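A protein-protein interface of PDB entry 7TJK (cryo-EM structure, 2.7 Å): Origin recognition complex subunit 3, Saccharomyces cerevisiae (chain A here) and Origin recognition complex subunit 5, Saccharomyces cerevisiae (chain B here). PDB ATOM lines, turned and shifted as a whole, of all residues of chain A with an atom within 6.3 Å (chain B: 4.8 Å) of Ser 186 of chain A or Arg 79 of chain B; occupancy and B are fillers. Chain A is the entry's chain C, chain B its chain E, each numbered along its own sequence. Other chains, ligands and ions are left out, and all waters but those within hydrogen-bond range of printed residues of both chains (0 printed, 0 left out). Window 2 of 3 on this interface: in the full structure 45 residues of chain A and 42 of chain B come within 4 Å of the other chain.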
ATOM      1  N   MET A 147      -2.018 -10.815  17.863  1.00  0.00           N
ATOM      2  CA  MET A 147      -3.448 -10.597  17.715  1.00  0.00           C
ATOM      3  C   MET A 147      -4.155 -11.849  17.224  1.00  0.00           C
ATOM      4  O   MET A 147      -5.311 -12.082  17.598  1.00  0.00           O
ATOM      5  CB  MET A 147      -3.715  -9.425  16.771  1.00  0.00           C
ATOM      6  CG  MET A 147      -3.330  -8.017  17.286  1.00  0.00           C
ATOM      7  SD  MET A 147      -4.160  -7.253  18.703  1.00  0.00           S
ATOM      8  CE  MET A 147      -3.282  -7.918  20.126  1.00  0.00           C
ATOM      9  N   SER A 182      -9.596  -8.065  11.608  1.00  0.00           N
ATOM     10  CA  SER A 182      -8.248  -7.792  11.128  1.00  0.00           C
ATOM     11  C   SER A 182      -7.262  -7.956  12.278  1.00  0.00           C
ATOM     12  O   SER A 182      -7.463  -7.392  13.359  1.00  0.00           O
ATOM     13  CB  SER A 182      -8.165  -6.382  10.544  1.00  0.00           C
ATOM     14  OG  SER A 182      -6.854  -6.088  10.101  1.00  0.00           O
ATOM     15  N   ASP A 184      -4.829  -6.990  14.235  1.00  0.00           N
ATOM     16  CA  ASP A 184      -4.363  -5.626  14.338  1.00  0.00           C
ATOM     17  C   ASP A 184      -4.809  -5.098  15.696  1.00  0.00           C
ATOM     18  O   ASP A 184      -5.712  -5.658  16.327  1.00  0.00           O
ATOM     19  CB  ASP A 184      -4.922  -4.821  13.159  1.00  0.00           C
ATOM     20  CG  ASP A 184      -4.304  -3.473  13.034  1.00  0.00           C
ATOM     21  OD1 ASP A 184      -3.060  -3.402  13.015  1.00  0.00           O
ATOM     22  OD2 ASP A 184      -5.062  -2.492  12.963  1.00  0.00           O
ATOM     23  N   LEU A 185      -4.199  -3.998  16.142  1.00  0.00           N
ATOM     24  CA  LEU A 185      -4.439  -3.456  17.477  1.00  0.00           C
ATOM     25  C   LEU A 185      -5.833  -2.848  17.641  1.00  0.00           C
ATOM     26  O   LEU A 185      -6.226  -2.532  18.770  1.00  0.00           O
ATOM     27  CB  LEU A 185      -3.362  -2.417  17.815  1.00  0.00           C
ATOM     28  CG  LEU A 185      -3.013  -2.191  19.293  1.00  0.00           C
ATOM     29  CD1 LEU A 185      -2.422  -3.451  19.908  1.00  0.00           C
ATOM     30  CD2 LEU A 185      -2.063  -1.021  19.468  1.00  0.00           C
ATOM     31  N   SER A 186      -6.597  -2.691  16.556  1.00  0.00           N
ATOM     32  CA  SER A 186      -7.998  -2.299  16.655  1.00  0.00           C
ATOM     33  C   SER A 186      -8.873  -3.384  17.272  1.00  0.00           C
ATOM     34  O   SER A 186      -9.987  -3.084  17.714  1.00  0.00           O
ATOM     35  CB  SER A 186      -8.538  -1.926  15.272  1.00  0.00           C
ATOM     36  OG  SER A 186      -8.495  -3.030  14.386  1.00  0.00           O
ATOM     37  N   LEU A 187      -8.409  -4.636  17.287  1.00  0.00           N
ATOM     38  CA  LEU A 187      -9.112  -5.692  18.008  1.00  0.00           C
ATOM     39  C   LEU A 187      -9.068  -5.461  19.515  1.00  0.00           C
ATOM     40  O   LEU A 187     -10.038  -5.770  20.218  1.00  0.00           O
ATOM     41  CB  LEU A 187      -8.510  -7.049  17.640  1.00  0.00           C
ATOM     42  CG  LEU A 187      -8.878  -8.290  18.449  1.00  0.00           C
ATOM     43  CD1 LEU A 187     -10.349  -8.618  18.266  1.00  0.00           C
ATOM     44  CD2 LEU A 187      -8.000  -9.460  18.042  1.00  0.00           C
ATOM     45  N   VAL A 188      -7.958  -4.918  20.020  1.00  0.00           N
ATOM     46  CA  VAL A 188      -7.867  -4.510  21.419  1.00  0.00           C
ATOM     47  C   VAL A 188      -8.831  -3.361  21.703  1.00  0.00           C
ATOM     48  O   VAL A 188      -9.451  -3.302  22.773  1.00  0.00           O
ATOM     49  CB  VAL A 188      -6.405  -4.145  21.751  1.00  0.00           C
ATOM     50  CG1 VAL A 188      -6.251  -3.624  23.163  1.00  0.00           C
ATOM     51  CG2 VAL A 188      -5.522  -5.344  21.562  1.00  0.00           C
ATOM     52  N   GLU A 189      -8.987  -2.449  20.736  1.00  0.00           N
ATOM     53  CA  GLU A 189      -9.929  -1.338  20.854  1.00  0.00           C
ATOM     54  C   GLU A 189     -11.371  -1.811  20.977  1.00  0.00           C
ATOM     55  O   GLU A 189     -12.134  -1.285  21.796  1.00  0.00           O
ATOM     56  CB  GLU A 189      -9.788  -0.416  19.643  1.00  0.00           C
ATOM     57  CG  GLU A 189     -10.355   0.967  19.838  1.00  0.00           C
ATOM     58  CD  GLU A 189     -10.492   1.724  18.537  1.00  0.00           C
ATOM     59  OE1 GLU A 189     -10.727   1.080  17.492  1.00  0.00           O
ATOM     60  OE2 GLU A 189     -10.357   2.965  18.557  1.00  0.00           O
ATOM     61  N   ASN A 190     -11.766  -2.795  20.175  1.00  0.00           N
ATOM     62  CA  ASN A 190     -13.141  -3.268  20.153  1.00  0.00           C
ATOM     63  C   ASN A 190     -13.321  -4.603  20.866  1.00  0.00           C
ATOM     64  O   ASN A 190     -14.242  -5.348  20.521  1.00  0.00           O
ATOM     65  CB  ASN A 190     -13.635  -3.375  18.709  1.00  0.00           C
ATOM     66  CG  ASN A 190     -13.609  -2.044  17.986  1.00  0.00           C
ATOM     67  OD1 ASN A 190     -14.127  -1.045  18.482  1.00  0.00           O
ATOM     68  ND2 ASN A 190     -13.008  -2.024  16.802  1.00  0.00           N
ATOM     69  N   PHE A 191     -12.469  -4.919  21.846  1.00  0.00           N
ATOM     70  CA  PHE A 191     -12.543  -6.222  22.502  1.00  0.00           C
ATOM     71  C   PHE A 191     -13.800  -6.352  23.358  1.00  0.00           C
ATOM     72  O   PHE A 191     -14.449  -7.406  23.355  1.00  0.00           O
ATOM     73  CB  PHE A 191     -11.290  -6.460  23.347  1.00  0.00           C
ATOM     74  CG  PHE A 191     -11.070  -7.903  23.709  1.00  0.00           C
ATOM     75  CD1 PHE A 191     -10.385  -8.745  22.847  1.00  0.00           C
ATOM     76  CD2 PHE A 191     -11.546  -8.417  24.908  1.00  0.00           C
ATOM     77  CE1 PHE A 191     -10.182 -10.074  23.169  1.00  0.00           C
ATOM     78  CE2 PHE A 191     -11.343  -9.745  25.236  1.00  0.00           C
ATOM     79  CZ  PHE A 191     -10.660 -10.573  24.365  1.00  0.00           C
ATOM     80  N   TYR A 229      -7.198   2.955  26.204  1.00  0.00           N
ATOM     81  CA  TYR A 229      -8.423   2.178  26.277  1.00  0.00           C
ATOM     82  C   TYR A 229      -8.640   1.720  27.714  1.00  0.00           C
ATOM     83  O   TYR A 229      -7.738   1.203  28.376  1.00  0.00           O
ATOM     84  CB  TYR A 229      -8.359   0.988  25.315  1.00  0.00           C
ATOM     85  CG  TYR A 229      -8.038   1.410  23.899  1.00  0.00           C
ATOM     86  CD1 TYR A 229      -8.661   2.515  23.328  1.00  0.00           C
ATOM     87  CD2 TYR A 229      -7.103   0.717  23.139  1.00  0.00           C
ATOM     88  CE1 TYR A 229      -8.361   2.920  22.047  1.00  0.00           C
ATOM     89  CE2 TYR A 229      -6.798   1.114  21.849  1.00  0.00           C
ATOM     90  CZ  TYR A 229      -7.433   2.217  21.310  1.00  0.00           C
ATOM     91  OH  TYR A 229      -7.145   2.617  20.027  1.00  0.00           O
ATOM     92  N   GLU B  66      -1.313   2.176  15.250  1.00  0.00           N
ATOM     93  CA  GLU B  66      -1.905   0.904  15.647  1.00  0.00           C
ATOM     94  C   GLU B  66      -2.118  -0.008  14.444  1.00  0.00           C
ATOM     95  O   GLU B  66      -2.023  -1.233  14.562  1.00  0.00           O
ATOM     96  CB  GLU B  66      -3.227   1.133  16.379  1.00  0.00           C
ATOM     97  CG  GLU B  66      -3.134   2.042  17.586  1.00  0.00           C
ATOM     98  CD  GLU B  66      -4.487   2.315  18.209  1.00  0.00           C
ATOM     99  OE1 GLU B  66      -5.206   1.340  18.516  1.00  0.00           O
ATOM    100  OE2 GLU B  66      -4.834   3.497  18.402  1.00  0.00           O
ATOM    101  N   GLN B  75      -8.799  -0.984   5.532  1.00  0.00           N
ATOM    102  CA  GLN B  75      -9.928  -1.666   6.159  1.00  0.00           C
ATOM    103  C   GLN B  75     -10.506  -0.855   7.315  1.00  0.00           C
ATOM    104  O   GLN B  75     -11.726  -0.834   7.515  1.00  0.00           O
ATOM    105  CB  GLN B  75      -9.502  -3.053   6.632  1.00  0.00           C
ATOM    106  CG  GLN B  75      -9.148  -4.003   5.507  1.00  0.00           C
ATOM    107  CD  GLN B  75      -8.364  -5.202   5.984  1.00  0.00           C
ATOM    108  OE1 GLN B  75      -7.912  -5.245   7.127  1.00  0.00           O
ATOM    109  NE2 GLN B  75      -8.191  -6.182   5.109  1.00  0.00           N
ATOM    110  N   ALA B  76      -9.647  -0.170   8.075  1.00  0.00           N
ATOM    111  CA  ALA B  76     -10.103   0.687   9.161  1.00  0.00           C
ATOM    112  C   ALA B  76     -10.866   1.897   8.645  1.00  0.00           C
ATOM    113  O   ALA B  76     -11.849   2.308   9.270  1.00  0.00           O
ATOM    114  CB  ALA B  76      -8.915   1.135  10.008  1.00  0.00           C
ATOM    115  N   ILE B  77     -10.428   2.472   7.518  1.00  0.00           N
ATOM    116  CA  ILE B  77     -11.170   3.569   6.894  1.00  0.00           C
ATOM    117  C   ILE B  77     -12.556   3.097   6.469  1.00  0.00           C
ATOM    118  O   ILE B  77     -13.571   3.735   6.784  1.00  0.00           O
ATOM    119  CB  ILE B  77     -10.378   4.146   5.703  1.00  0.00           C
ATOM    120  CG1 ILE B  77      -9.195   4.977   6.199  1.00  0.00           C
ATOM    121  CG2 ILE B  77     -11.269   4.997   4.800  1.00  0.00           C
ATOM    122  CD1 ILE B  77      -8.147   5.231   5.147  1.00  0.00           C
ATOM    123  N   ALA B  78     -12.617   1.932   5.810  1.00  0.00           N
ATOM    124  CA  ALA B  78     -13.891   1.390   5.338  1.00  0.00           C
ATOM    125  C   ALA B  78     -14.834   1.032   6.484  1.00  0.00           C
ATOM    126  O   ALA B  78     -16.049   1.225   6.367  1.00  0.00           O
ATOM    127  CB  ALA B  78     -13.642   0.166   4.458  1.00  0.00           C
ATOM    128  N   ARG B  79     -14.299   0.519   7.595  1.00  0.00           N
ATOM    129  CA  ARG B  79     -15.135   0.205   8.751  1.00  0.00           C
ATOM    130  C   ARG B  79     -15.637   1.468   9.443  1.00  0.00           C
ATOM    131  O   ARG B  79     -16.841   1.614   9.701  1.00  0.00           O
ATOM    132  CB  ARG B  79     -14.347  -0.661   9.735  1.00  0.00           C
ATOM    133  CG  ARG B  79     -15.063  -0.947  11.041  1.00  0.00           C
ATOM    134  CD  ARG B  79     -14.368  -2.049  11.823  1.00  0.00           C
ATOM    135  NE  ARG B  79     -13.100  -1.606  12.389  1.00  0.00           N
ATOM    136  CZ  ARG B  79     -11.910  -1.966  11.929  1.00  0.00           C
ATOM    137  NH1 ARG B  79     -11.787  -2.787  10.899  1.00  0.00           N
ATOM    138  NH2 ARG B  79     -10.815  -1.485  12.512  1.00  0.00           N
ATOM    139  N   THR B  80     -14.728   2.404   9.731  1.00  0.00           N
ATOM    140  CA  THR B  80     -15.074   3.521  10.599  1.00  0.00           C
ATOM    141  C   THR B  80     -15.917   4.570   9.885  1.00  0.00           C
ATOM    142  O   THR B  80     -16.752   5.215  10.533  1.00  0.00           O
ATOM    143  CB  THR B  80     -13.804   4.140  11.177  1.00  0.00           C
ATOM    144  OG1 THR B  80     -12.871   4.405  10.121  1.00  0.00           O
ATOM    145  CG2 THR B  80     -13.167   3.209  12.195  1.00  0.00           C
ATOM    146  N   VAL B  81     -15.751   4.726   8.563  1.00  0.00           N
ATOM    147  CA  VAL B  81     -16.578   5.669   7.811  1.00  0.00           C
ATOM    148  C   VAL B  81     -18.042   5.236   7.831  1.00  0.00           C
ATOM    149  O   VAL B  81     -18.936   6.034   8.140  1.00  0.00           O
ATOM    150  CB  VAL B  81     -16.045   5.822   6.373  1.00  0.00           C
ATOM    151  CG1 VAL B  81     -17.115   6.363   5.433  1.00  0.00           C
ATOM    152  CG2 VAL B  81     -14.842   6.739   6.357  1.00  0.00           C
ATOM    153  N   GLN B  82     -18.303   3.955   7.568  1.00  0.00           N
ATOM    154  CA  GLN B  82     -19.682   3.492   7.572  1.00  0.00           C
ATOM    155  C   GLN B  82     -20.259   3.357   8.977  1.00  0.00           C
ATOM    156  O   GLN B  82     -21.467   3.550   9.140  1.00  0.00           O
ATOM    157  CB  GLN B  82     -19.816   2.176   6.795  1.00  0.00           C
ATOM    158  CG  GLN B  82     -19.217   0.947   7.437  1.00  0.00           C
ATOM    159  CD  GLN B  82     -19.492  -0.308   6.633  1.00  0.00           C
ATOM    160  OE1 GLN B  82     -20.525  -0.423   5.974  1.00  0.00           O
ATOM    161  NE2 GLN B  82     -18.562  -1.254   6.676  1.00  0.00           N
ATOM    162  N   TYR B  83     -19.432   3.088   9.999  1.00  0.00           N
ATOM    163  CA  TYR B  83     -19.955   3.102  11.366  1.00  0.00           C
ATOM    164  C   TYR B  83     -20.356   4.516  11.784  1.00  0.00           C
ATOM    165  O   TYR B  83     -21.409   4.705  12.410  1.00  0.00           O
ATOM    166  CB  TYR B  83     -18.931   2.469  12.327  1.00  0.00           C
ATOM    167  CG  TYR B  83     -19.235   2.520  13.829  1.00  0.00           C
ATOM    168  CD1 TYR B  83     -18.971   3.653  14.606  1.00  0.00           C
ATOM    169  CD2 TYR B  83     -19.826   1.430  14.459  1.00  0.00           C
ATOM    170  CE1 TYR B  83     -19.264   3.685  15.954  1.00  0.00           C
ATOM    171  CE2 TYR B  83     -20.122   1.454  15.808  1.00  0.00           C
ATOM    172  CZ  TYR B  83     -19.839   2.582  16.550  1.00  0.00           C
ATOM    173  OH  TYR B  83     -20.133   2.609  17.894  1.00  0.00           O
ATOM    174  N   PRO B  99     -15.758  -4.361   5.709  1.00  0.00           N
ATOM    175  CA  PRO B  99     -14.461  -3.686   5.524  1.00  0.00           C
ATOM    176  C   PRO B  99     -13.332  -4.624   5.130  1.00  0.00           C
ATOM    177  O   PRO B  99     -12.310  -4.154   4.619  1.00  0.00           O
ATOM    178  CB  PRO B  99     -14.199  -3.043   6.892  1.00  0.00           C
ATOM    179  CG  PRO B  99     -15.043  -3.813   7.848  1.00  0.00           C
ATOM    180  CD  PRO B  99     -16.260  -4.226   7.086  1.00  0.00           C
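The side-chain carboxylate of Glu 66 of chain B lies within hydrogen-bond range of the side-chain hydroxyl of Tyr 229 of chain A. The side-chain hydroxyl of Ser 182 of chain A lies within hydrogen-bond range of the side-chain amide oxygen of Gln 75 of chain B. The guanidinium group of Arg 79 of chain B lies within hydrogen-bond range of the side-chain hydroxyl of Ser 186 of chain A (3.4 Å). The side-chain carboxylate (OD1) of Asp 184 of chain A sits close to the backbone carbonyl oxygen (O) of Glu 66 of chain B (2.9 Å).
The backbone carbonyl oxygen (O) of Ser 186 of chain A sits at hydrogen-bond distance from the side-chain amide nitrogen (ND2) of Asn 190 of chain A (3.3 Å).
Among the printed residues, merely in contact across the chains: Leu 185 of chain A with Glu 66 of chain B.
Of the printed residues of chain B, Asp 184 of chain A touches Glu 66. Printed residues of chain B within 4 Å of Leu 185 of chain A: Glu 66 (3.7 Å). Ser 186 of chain A touches just one residue of chain B: Arg 79. Glu 189 of chain A touches none of the printed residues of chain B. Of the printed residues of chain B, Tyr 229 of chain A touches Glu 66. Printed residues of chain A within 4 Å of Glu 66 of chain B: Asp 184 (2.9 Å), Leu 185 (3.7 Å) and Tyr 229 (2.8 Å). Of the printed residues of chain A, Gln 75 of chain B touches Ser 182 (3.3 Å). Arg 79 of chain B touches one residue of chain A. The nearest residue of chain B that does not touch Ser 186 of chain A is Glu 66 of chain B (4.7 Å). The nearest residue of chain A that does not touch Arg 79 of chain B is Asn 190 of chain A (4.4 Å). The nearest printed residue of chain B that does not touch Ser 182 of chain A is Arg 79 of chain B (5.1 Å).
Of the 11 printed residues of chain A, 5 touch a printed residue of chain B. Hydrophobic or aromatic side chains of chain A that line the printed part of chain B: Leu 185 and Tyr 229. Along chain B the printed residues that touch a printed residue of chain A span positions 66 to 79.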
